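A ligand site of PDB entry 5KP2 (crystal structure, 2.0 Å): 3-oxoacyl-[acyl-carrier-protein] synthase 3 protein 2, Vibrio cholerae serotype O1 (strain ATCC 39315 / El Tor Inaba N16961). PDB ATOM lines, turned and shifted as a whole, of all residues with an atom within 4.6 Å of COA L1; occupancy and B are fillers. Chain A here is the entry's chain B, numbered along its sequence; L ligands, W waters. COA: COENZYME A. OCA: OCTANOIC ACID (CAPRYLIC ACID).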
ATOM      1  N   ASP A  30     -12.558 -23.808 -19.230  1.00  0.00           N
ATOM      2  CA  ASP A  30     -13.020 -24.380 -17.963  1.00  0.00           C
ATOM      3  C   ASP A  30     -13.448 -23.248 -17.029  1.00  0.00           C
ATOM      4  O   ASP A  30     -12.699 -22.828 -16.149  1.00  0.00           O
ATOM      5  CB  ASP A  30     -11.946 -25.255 -17.310  1.00  0.00           C
ATOM      6  CG  ASP A  30     -12.404 -25.839 -15.980  1.00  0.00           C
ATOM      7  OD1 ASP A  30     -13.583 -26.229 -15.849  1.00  0.00           O
ATOM      8  OD2 ASP A  30     -11.584 -25.899 -15.054  1.00  0.00           O
ATOM      9  N   THR A  31     -14.652 -22.740 -17.256  1.00  0.00           N
ATOM     10  CA  THR A  31     -15.206 -21.656 -16.462  1.00  0.00           C
ATOM     11  C   THR A  31     -16.719 -21.813 -16.371  1.00  0.00           C
ATOM     12  O   THR A  31     -17.291 -22.704 -17.005  1.00  0.00           O
ATOM     13  CB  THR A  31     -14.814 -20.278 -17.051  1.00  0.00           C
ATOM     14  OG1 THR A  31     -15.215 -19.222 -16.163  1.00  0.00           O
ATOM     15  CG2 THR A  31     -15.421 -20.060 -18.435  1.00  0.00           C
ATOM     16  N   TRP A  35     -19.029 -18.517 -11.532  1.00  0.00           N
ATOM     17  CA  TRP A  35     -17.759 -17.973 -11.069  1.00  0.00           C
ATOM     18  C   TRP A  35     -17.515 -16.550 -11.594  1.00  0.00           C
ATOM     19  O   TRP A  35     -17.117 -15.654 -10.829  1.00  0.00           O
ATOM     20  CB  TRP A  35     -16.568 -18.861 -11.429  1.00  0.00           C
ATOM     21  CG  TRP A  35     -15.333 -18.287 -10.803  1.00  0.00           C
ATOM     22  CD1 TRP A  35     -14.842 -18.562  -9.556  1.00  0.00           C
ATOM     23  CD2 TRP A  35     -14.491 -17.260 -11.356  1.00  0.00           C
ATOM     24  NE1 TRP A  35     -13.731 -17.792  -9.317  1.00  0.00           N
ATOM     25  CE2 TRP A  35     -13.492 -16.976 -10.393  1.00  0.00           C
ATOM     26  CE3 TRP A  35     -14.485 -16.559 -12.563  1.00  0.00           C
ATOM     27  CZ2 TRP A  35     -12.481 -16.030 -10.615  1.00  0.00           C
ATOM     28  CZ3 TRP A  35     -13.476 -15.604 -12.781  1.00  0.00           C
ATOM     29  CH2 TRP A  35     -12.498 -15.349 -11.808  1.00  0.00           C
ATOM     30  N   ARG A  39     -17.198 -13.415  -9.231  1.00  0.00           N
ATOM     31  CA  ARG A  39     -15.836 -12.874  -9.063  1.00  0.00           C
ATOM     32  C   ARG A  39     -15.613 -11.516  -9.743  1.00  0.00           C
ATOM     33  O   ARG A  39     -14.972 -10.638  -9.159  1.00  0.00           O
ATOM     34  CB  ARG A  39     -14.799 -13.866  -9.598  1.00  0.00           C
ATOM     35  N   THR A  40     -16.110 -11.366 -10.976  1.00  0.00           N
ATOM     36  CA  THR A  40     -15.899 -10.149 -11.776  1.00  0.00           C
ATOM     37  C   THR A  40     -17.137  -9.235 -11.861  1.00  0.00           C
ATOM     38  O   THR A  40     -16.994  -8.006 -11.973  1.00  0.00           O
ATOM     39  CB  THR A  40     -15.414 -10.474 -13.216  1.00  0.00           C
ATOM     40  OG1 THR A  40     -16.489 -10.985 -14.016  1.00  0.00           O
ATOM     41  CG2 THR A  40     -14.275 -11.494 -13.189  1.00  0.00           C
ATOM     42  N   ARG A 152      -8.309 -18.661 -19.343  1.00  0.00           N
ATOM     43  CA  ARG A 152      -9.550 -18.162 -18.751  1.00  0.00           C
ATOM     44  C   ARG A 152      -9.355 -16.893 -17.901  1.00  0.00           C
ATOM     45  O   ARG A 152     -10.286 -16.097 -17.774  1.00  0.00           O
ATOM     46  CB  ARG A 152     -10.233 -19.262 -17.922  1.00  0.00           C
ATOM     47  CG  ARG A 152      -9.512 -19.640 -16.631  1.00  0.00           C
ATOM     48  CD  ARG A 152     -10.174 -20.808 -15.929  1.00  0.00           C
ATOM     49  NE  ARG A 152      -9.620 -20.987 -14.588  1.00  0.00           N
ATOM     50  CZ  ARG A 152     -10.072 -21.830 -13.664  1.00  0.00           C
ATOM     51  NH1 ARG A 152     -11.108 -22.638 -13.910  1.00  0.00           N
ATOM     52  NH2 ARG A 152      -9.471 -21.891 -12.470  1.00  0.00           N
ATOM     53  N   ASP A 153      -8.170 -16.716 -17.312  1.00  0.00           N
ATOM     54  CA  ASP A 153      -7.847 -15.551 -16.464  1.00  0.00           C
ATOM     55  C   ASP A 153      -8.152 -14.234 -17.155  1.00  0.00           C
ATOM     56  O   ASP A 153      -8.834 -13.366 -16.602  1.00  0.00           O
ATOM     57  CB  ASP A 153      -6.356 -15.562 -16.058  1.00  0.00           C
ATOM     58  N   VAL A 156     -11.942 -13.753 -20.155  1.00  0.00           N
ATOM     59  CA  VAL A 156     -13.268 -13.399 -19.684  1.00  0.00           C
ATOM     60  C   VAL A 156     -13.446 -11.901 -19.315  1.00  0.00           C
ATOM     61  O   VAL A 156     -14.564 -11.494 -19.055  1.00  0.00           O
ATOM     62  CB  VAL A 156     -13.715 -14.288 -18.487  1.00  0.00           C
ATOM     63  CG1 VAL A 156     -13.542 -15.771 -18.812  1.00  0.00           C
ATOM     64  CG2 VAL A 156     -12.969 -13.955 -17.202  1.00  0.00           C
ATOM     65  N   PHE A 158     -12.261  -8.803 -21.030  1.00  0.00           N
ATOM     66  CA  PHE A 158     -12.157  -7.704 -22.005  1.00  0.00           C
ATOM     67  C   PHE A 158     -13.195  -7.783 -23.104  1.00  0.00           C
ATOM     68  O   PHE A 158     -13.612  -8.872 -23.503  1.00  0.00           O
ATOM     69  CB  PHE A 158     -10.744  -7.657 -22.636  1.00  0.00           C
ATOM     70  CG  PHE A 158      -9.659  -7.460 -21.630  1.00  0.00           C
ATOM     71  CD1 PHE A 158      -9.402  -6.192 -21.122  1.00  0.00           C
ATOM     72  CD2 PHE A 158      -8.915  -8.542 -21.172  1.00  0.00           C
ATOM     73  CE1 PHE A 158      -8.412  -6.001 -20.174  1.00  0.00           C
ATOM     74  CE2 PHE A 158      -7.923  -8.361 -20.227  1.00  0.00           C
ATOM     75  CZ  PHE A 158      -7.663  -7.085 -19.739  1.00  0.00           C
ATOM     76  N   LEU A 191       1.487  -5.307 -16.304  1.00  0.00           N
ATOM     77  CA  LEU A 191       0.368  -5.366 -17.264  1.00  0.00           C
ATOM     78  C   LEU A 191       0.918  -4.971 -18.625  1.00  0.00           C
ATOM     79  O   LEU A 191       1.224  -3.786 -18.855  1.00  0.00           O
ATOM     80  CB  LEU A 191      -0.739  -4.398 -16.844  1.00  0.00           C
ATOM     81  CG  LEU A 191      -2.013  -4.292 -17.684  1.00  0.00           C
ATOM     82  CD1 LEU A 191      -2.784  -5.607 -17.745  1.00  0.00           C
ATOM     83  CD2 LEU A 191      -2.895  -3.209 -17.085  1.00  0.00           C
ATOM     84  N   PHE A 214       0.980 -10.047 -16.350  1.00  0.00           N
ATOM     85  CA  PHE A 214      -0.220  -9.731 -15.569  1.00  0.00           C
ATOM     86  C   PHE A 214       0.033 -10.173 -14.112  1.00  0.00           C
ATOM     87  O   PHE A 214       0.228 -11.349 -13.853  1.00  0.00           O
ATOM     88  CB  PHE A 214      -1.444 -10.448 -16.153  1.00  0.00           C
ATOM     89  CG  PHE A 214      -2.747 -10.037 -15.531  1.00  0.00           C
ATOM     90  CD1 PHE A 214      -3.232 -10.682 -14.398  1.00  0.00           C
ATOM     91  CD2 PHE A 214      -3.502  -8.997 -16.085  1.00  0.00           C
ATOM     92  CE1 PHE A 214      -4.440 -10.308 -13.832  1.00  0.00           C
ATOM     93  CE2 PHE A 214      -4.716  -8.618 -15.509  1.00  0.00           C
ATOM     94  CZ  PHE A 214      -5.178  -9.269 -14.375  1.00  0.00           C
ATOM     95  N   GLY A 216      -2.166  -9.344 -10.939  1.00  0.00           N
ATOM     96  CA  GLY A 216      -3.428  -8.729 -10.555  1.00  0.00           C
ATOM     97  C   GLY A 216      -3.463  -7.926  -9.269  1.00  0.00           C
ATOM     98  O   GLY A 216      -4.067  -6.854  -9.221  1.00  0.00           O
ATOM     99  N   LYS A 217      -2.836  -8.442  -8.208  1.00  0.00           N
ATOM    100  CA  LYS A 217      -2.823  -7.742  -6.913  1.00  0.00           C
ATOM    101  C   LYS A 217      -1.948  -6.478  -6.923  1.00  0.00           C
ATOM    102  O   LYS A 217      -2.258  -5.499  -6.248  1.00  0.00           O
ATOM    103  CB  LYS A 217      -2.378  -8.685  -5.787  1.00  0.00           C
ATOM    104  CG  LYS A 217      -3.389  -9.782  -5.509  1.00  0.00           C
ATOM    105  CD  LYS A 217      -2.967 -10.669  -4.343  1.00  0.00           C
ATOM    106  CE  LYS A 217      -3.982 -11.766  -4.095  1.00  0.00           C
ATOM    107  NZ  LYS A 217      -3.701 -12.499  -2.832  1.00  0.00           N
ATOM    108  N   ILE A 219      -1.469  -4.705  -9.774  1.00  0.00           N
ATOM    109  CA  ILE A 219      -2.290  -3.774 -10.563  1.00  0.00           C
ATOM    110  C   ILE A 219      -3.314  -3.105  -9.650  1.00  0.00           C
ATOM    111  O   ILE A 219      -3.468  -1.876  -9.681  1.00  0.00           O
ATOM    112  CB  ILE A 219      -3.026  -4.450 -11.736  1.00  0.00           C
ATOM    113  CG1 ILE A 219      -2.026  -4.968 -12.775  1.00  0.00           C
ATOM    114  CG2 ILE A 219      -3.982  -3.473 -12.426  1.00  0.00           C
ATOM    115  CD1 ILE A 219      -2.566  -6.075 -13.655  1.00  0.00           C
ATOM    116  N   PHE A 220      -3.999  -3.904  -8.843  1.00  0.00           N
ATOM    117  CA  PHE A 220      -5.003  -3.393  -7.904  1.00  0.00           C
ATOM    118  C   PHE A 220      -4.411  -2.264  -7.028  1.00  0.00           C
ATOM    119  O   PHE A 220      -4.954  -1.170  -6.980  1.00  0.00           O
ATOM    120  CB  PHE A 220      -5.536  -4.549  -7.051  1.00  0.00           C
ATOM    121  CG  PHE A 220      -6.729  -4.173  -6.222  1.00  0.00           C
ATOM    122  CD1 PHE A 220      -6.576  -3.506  -5.029  1.00  0.00           C
ATOM    123  CD2 PHE A 220      -8.008  -4.531  -6.637  1.00  0.00           C
ATOM    124  CE1 PHE A 220      -7.680  -3.166  -4.262  1.00  0.00           C
ATOM    125  CE2 PHE A 220      -9.116  -4.187  -5.882  1.00  0.00           C
ATOM    126  CZ  PHE A 220      -8.945  -3.503  -4.696  1.00  0.00           C
ATOM    127  N   ALA A 253     -12.752  -1.625 -15.130  1.00  0.00           N
ATOM    128  CA  ALA A 253     -11.834  -2.772 -15.165  1.00  0.00           C
ATOM    129  C   ALA A 253     -12.160  -3.829 -14.127  1.00  0.00           C
ATOM    130  O   ALA A 253     -12.003  -5.012 -14.364  1.00  0.00           O
ATOM    131  CB  ALA A 253     -10.400  -2.304 -14.969  1.00  0.00           C
ATOM    132  N   ASN A 254     -12.598  -3.372 -12.958  1.00  0.00           N
ATOM    133  CA  ASN A 254     -12.822  -4.255 -11.839  1.00  0.00           C
ATOM    134  C   ASN A 254     -13.711  -3.492 -10.849  1.00  0.00           C
ATOM    135  O   ASN A 254     -13.415  -2.336 -10.515  1.00  0.00           O
ATOM    136  CB  ASN A 254     -11.469  -4.639 -11.230  1.00  0.00           C
ATOM    137  CG  ASN A 254     -11.595  -5.546 -10.026  1.00  0.00           C
ATOM    138  OD1 ASN A 254     -11.762  -5.078  -8.898  1.00  0.00           O
ATOM    139  ND2 ASN A 254     -11.541  -6.841 -10.247  1.00  0.00           N
ATOM    140  N   ARG A 256     -14.333  -4.074  -7.601  1.00  0.00           N
ATOM    141  CA  ARG A 256     -13.711  -3.869  -6.270  1.00  0.00           C
ATOM    142  C   ARG A 256     -12.739  -2.671  -6.285  1.00  0.00           C
ATOM    143  O   ARG A 256     -12.626  -1.974  -5.279  1.00  0.00           O
ATOM    144  CB  ARG A 256     -13.011  -5.125  -5.745  1.00  0.00           C
ATOM    145  CG  ARG A 256     -13.943  -6.254  -5.282  1.00  0.00           C
ATOM    146  CD  ARG A 256     -14.633  -5.970  -3.955  1.00  0.00           C
ATOM    147  NE  ARG A 256     -14.581  -7.120  -3.054  1.00  0.00           N
ATOM    148  CZ  ARG A 256     -15.300  -8.235  -3.189  1.00  0.00           C
ATOM    149  NH1 ARG A 256     -15.175  -9.213  -2.308  1.00  0.00           N
ATOM    150  NH2 ARG A 256     -16.142  -8.382  -4.209  1.00  0.00           N
ATOM    151  N   ILE A 257     -12.074  -2.437  -7.419  1.00  0.00           N
ATOM    152  CA  ILE A 257     -11.242  -1.232  -7.584  1.00  0.00           C
ATOM    153  C   ILE A 257     -12.081   0.037  -7.457  1.00  0.00           C
ATOM    154  O   ILE A 257     -11.694   0.954  -6.728  1.00  0.00           O
ATOM    155  CB  ILE A 257     -10.456  -1.224  -8.919  1.00  0.00           C
ATOM    156  CG1 ILE A 257      -9.322  -2.261  -8.851  1.00  0.00           C
ATOM    157  CG2 ILE A 257      -9.873   0.151  -9.201  1.00  0.00           C
ATOM    158  CD1 ILE A 257      -8.577  -2.464 -10.164  1.00  0.00           C
ATOM    159  N   ASN A 281     -14.297  -4.923 -19.765  1.00  0.00           N
ATOM    160  CA  ASN A 281     -13.279  -3.854 -19.879  1.00  0.00           C
ATOM    161  C   ASN A 281     -13.031  -3.580 -21.357  1.00  0.00           C
ATOM    162  O   ASN A 281     -12.506  -4.425 -22.051  1.00  0.00           O
ATOM    163  CB  ASN A 281     -11.991  -4.301 -19.162  1.00  0.00           C
ATOM    164  CG  ASN A 281     -10.873  -3.237 -19.154  1.00  0.00           C
ATOM    165  OD1 ASN A 281     -10.893  -2.255 -19.905  1.00  0.00           O
ATOM    166  ND2 ASN A 281      -9.865  -3.464 -18.326  1.00  0.00           N
ATOM    167  N   PHE A 311      -7.294   4.329 -15.021  1.00  0.00           N
ATOM    168  CA  PHE A 311      -5.933   3.810 -15.006  1.00  0.00           C
ATOM    169  C   PHE A 311      -5.776   2.826 -16.151  1.00  0.00           C
ATOM    170  O   PHE A 311      -6.766   2.346 -16.701  1.00  0.00           O
ATOM    171  CB  PHE A 311      -5.628   3.109 -13.670  1.00  0.00           C
ATOM    172  CG  PHE A 311      -6.276   1.752 -13.558  1.00  0.00           C
ATOM    173  CD1 PHE A 311      -7.590   1.638 -13.131  1.00  0.00           C
ATOM    174  CD2 PHE A 311      -5.577   0.597 -13.913  1.00  0.00           C
ATOM    175  CE1 PHE A 311      -8.203   0.394 -13.043  1.00  0.00           C
ATOM    176  CE2 PHE A 311      -6.189  -0.661 -13.845  1.00  0.00           C
ATOM    177  CZ  PHE A 311      -7.501  -0.748 -13.402  1.00  0.00           C
HETATM  178  N1A COA L   1     -13.102 -19.596 -13.891  1.00  0.00           N
HETATM  179  C2A COA L   1     -13.018 -20.184 -12.681  1.00  0.00           C
HETATM  180  N3A COA L   1     -12.123 -19.815 -11.736  1.00  0.00           N
HETATM  181  C4A COA L   1     -11.238 -18.805 -11.962  1.00  0.00           C
HETATM  182  C5A COA L   1     -11.264 -18.117 -13.265  1.00  0.00           C
HETATM  183  C6A COA L   1     -12.282 -18.580 -14.252  1.00  0.00           C
HETATM  184  N6A COA L   1     -12.349 -17.976 -15.468  1.00  0.00           N
HETATM  185  N7A COA L   1     -10.304 -17.178 -13.234  1.00  0.00           N
HETATM  186  C8A COA L   1      -9.706 -17.247 -12.019  1.00  0.00           C
HETATM  187  N9A COA L   1     -10.252 -18.221 -11.255  1.00  0.00           N
HETATM  188  C1B COA L   1      -9.893 -18.620  -9.861  1.00  0.00           C
HETATM  189  C2B COA L   1      -8.403 -18.485  -9.528  1.00  0.00           C
HETATM  190  O2B COA L   1      -7.742 -19.751  -9.607  1.00  0.00           O
HETATM  191  C3B COA L   1      -8.354 -17.879  -8.135  1.00  0.00           C
HETATM  192  O3B COA L   1      -7.863 -18.800  -7.164  1.00  0.00           O
HETATM  193  P3B COA L   1      -6.321 -18.719  -6.716  1.00  0.00           P
HETATM  194  O7A COA L   1      -6.110 -19.985  -5.919  1.00  0.00           O
HETATM  195  O8A COA L   1      -6.252 -17.445  -5.913  1.00  0.00           O
HETATM  196  O9A COA L   1      -5.571 -18.672  -8.030  1.00  0.00           O
HETATM  197  C4B COA L   1      -9.778 -17.440  -7.797  1.00  0.00           C
HETATM  198  O4B COA L   1     -10.610 -17.832  -8.908  1.00  0.00           O
HETATM  199  C5B COA L   1      -9.903 -15.941  -7.577  1.00  0.00           C
HETATM  200  O5B COA L   1      -9.325 -15.236  -8.680  1.00  0.00           O
HETATM  201  P1A COA L   1      -9.035 -13.652  -8.653  1.00  0.00           P
HETATM  202  O1A COA L   1      -7.920 -13.375  -9.644  1.00  0.00           O
HETATM  203  O2A COA L   1      -8.905 -13.200  -7.214  1.00  0.00           O
HETATM  204  O3A COA L   1     -10.405 -13.083  -9.273  1.00  0.00           O
HETATM  205  P2A COA L   1     -10.571 -11.526  -9.664  1.00  0.00           P
HETATM  206  O4A COA L   1     -12.027 -11.273  -9.974  1.00  0.00           O
HETATM  207  O5A COA L   1      -9.519 -11.155 -10.678  1.00  0.00           O
HETATM  208  O6A COA L   1     -10.194 -10.791  -8.277  1.00  0.00           O
HETATM  209  CBP COA L   1     -10.192  -8.827  -6.773  1.00  0.00           C
HETATM  210  CCP COA L   1     -10.706  -9.485  -8.058  1.00  0.00           C
HETATM  211  CDP COA L   1     -11.266  -7.819  -6.415  1.00  0.00           C
HETATM  212  CEP COA L   1     -10.070  -9.819  -5.622  1.00  0.00           C
HETATM  213  CAP COA L   1      -8.896  -7.998  -6.944  1.00  0.00           C
HETATM  214  OAP COA L   1      -8.251  -7.774  -5.680  1.00  0.00           O
HETATM  215  C9P COA L   1      -7.899  -8.630  -7.884  1.00  0.00           C
HETATM  216  O9P COA L   1      -7.098  -9.458  -7.468  1.00  0.00           O
HETATM  217  N8P COA L   1      -7.959  -8.203  -9.145  1.00  0.00           N
HETATM  218  C7P COA L   1      -7.035  -8.669 -10.158  1.00  0.00           C
HETATM  219  C6P COA L   1      -7.003  -7.846 -11.445  1.00  0.00           C
HETATM  220  C5P COA L   1      -7.148  -6.342 -11.249  1.00  0.00           C
HETATM  221  O5P COA L   1      -7.199  -5.897 -10.116  1.00  0.00           O
HETATM  222  N4P COA L   1      -7.208  -5.524 -12.311  1.00  0.00           N
HETATM  223  C3P COA L   1      -7.133  -5.951 -13.710  1.00  0.00           C
HETATM  224  C2P COA L   1      -7.507  -4.852 -14.694  1.00  0.00           C
HETATM  225  S1P COA L   1      -6.484  -4.914 -16.189  1.00  0.00           S
HETATM  226  C1  OCA L   2      -6.445  -1.522 -19.593  1.00  0.00           C
HETATM  227  C2  OCA L   2      -6.538  -2.655 -20.581  1.00  0.00           C
HETATM  228  C3  OCA L   2      -5.270  -2.880 -21.399  1.00  0.00           C
HETATM  229  C4  OCA L   2      -5.076  -4.348 -21.754  1.00  0.00           C
HETATM  230  C5  OCA L   2      -6.018  -4.803 -22.869  1.00  0.00           C
HETATM  231  C6  OCA L   2      -6.129  -6.323 -22.976  1.00  0.00           C
HETATM  232  C7  OCA L   2      -5.134  -6.916 -23.963  1.00  0.00           C
HETATM  233  C8  OCA L   2      -4.694  -8.305 -23.532  1.00  0.00           C
HETATM  234  O1  OCA L   2      -7.159  -1.585 -18.566  1.00  0.00           O
HETATM  235  O2  OCA L   2      -5.679  -0.574 -19.828  1.00  0.00           O
HETATM  236  O   HOH W   1      -9.227 -21.962  -9.343  1.00  0.00           O
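The indole nitrogen of Trp 35 lies close to an oxygen (O4B) of COA L1 (3.1 Å).
ND2 of Asn 281 sits at hydrogen-bond distance from O1 of OCA L2, at 3.3 Å.
The guanidinium group of Arg 152 sits at hydrogen-bond distance from a nitrogen (N3A) of COA L1 (3.4 Å).
N1A of COA L1 is in hydrogen-bond range of OG1 of Thr 31 (3.1 Å).
The guanidinium group (NH1) of Arg 152 is in salt-bridge range of the side-chain carboxylate (OD2) of Asp 30, at 3.5 Å.
The side-chain amide oxygen (OD1) of Asn 254 lies within hydrogen-bond range of the backbone NH (N) of Ile 257, 3.0 Å away.
The side-chain amide oxygen (OD1) of Asn 254 sits at hydrogen-bond distance from the backbone NH (N) of Arg 256, 3.0 Å away.
O4A of COA L1 sits close to O of Arg 39, at 3.1 Å.
O of Gly 216 sits close to O5P of COA L1, at 3.4 Å.
Asp 30 touches COA L1 (O to N1A, 3.96 Å).
CG2 of Thr 40 touches O4A of COA L1, 3.9 Å away.
Phe 214 touches COA L1 (CZ to C6P, 3.7 Å).
CG2 of Ile 219 touches N4P of COA L1, at 3.8 Å.
Phe 220 touches COA L1 (CD2 to OAP, 3.4 Å).
Ala 253 touches COA L1.
Asn 254 touches COA L1.
Arg 256 touches COA L1.
Ile 257 touches COA L1.
Of the 21 residues printed, 14 come within 4 Å of COA L1.
Water W1 bridges O2B of COA L1 and NH2 of Arg 152.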
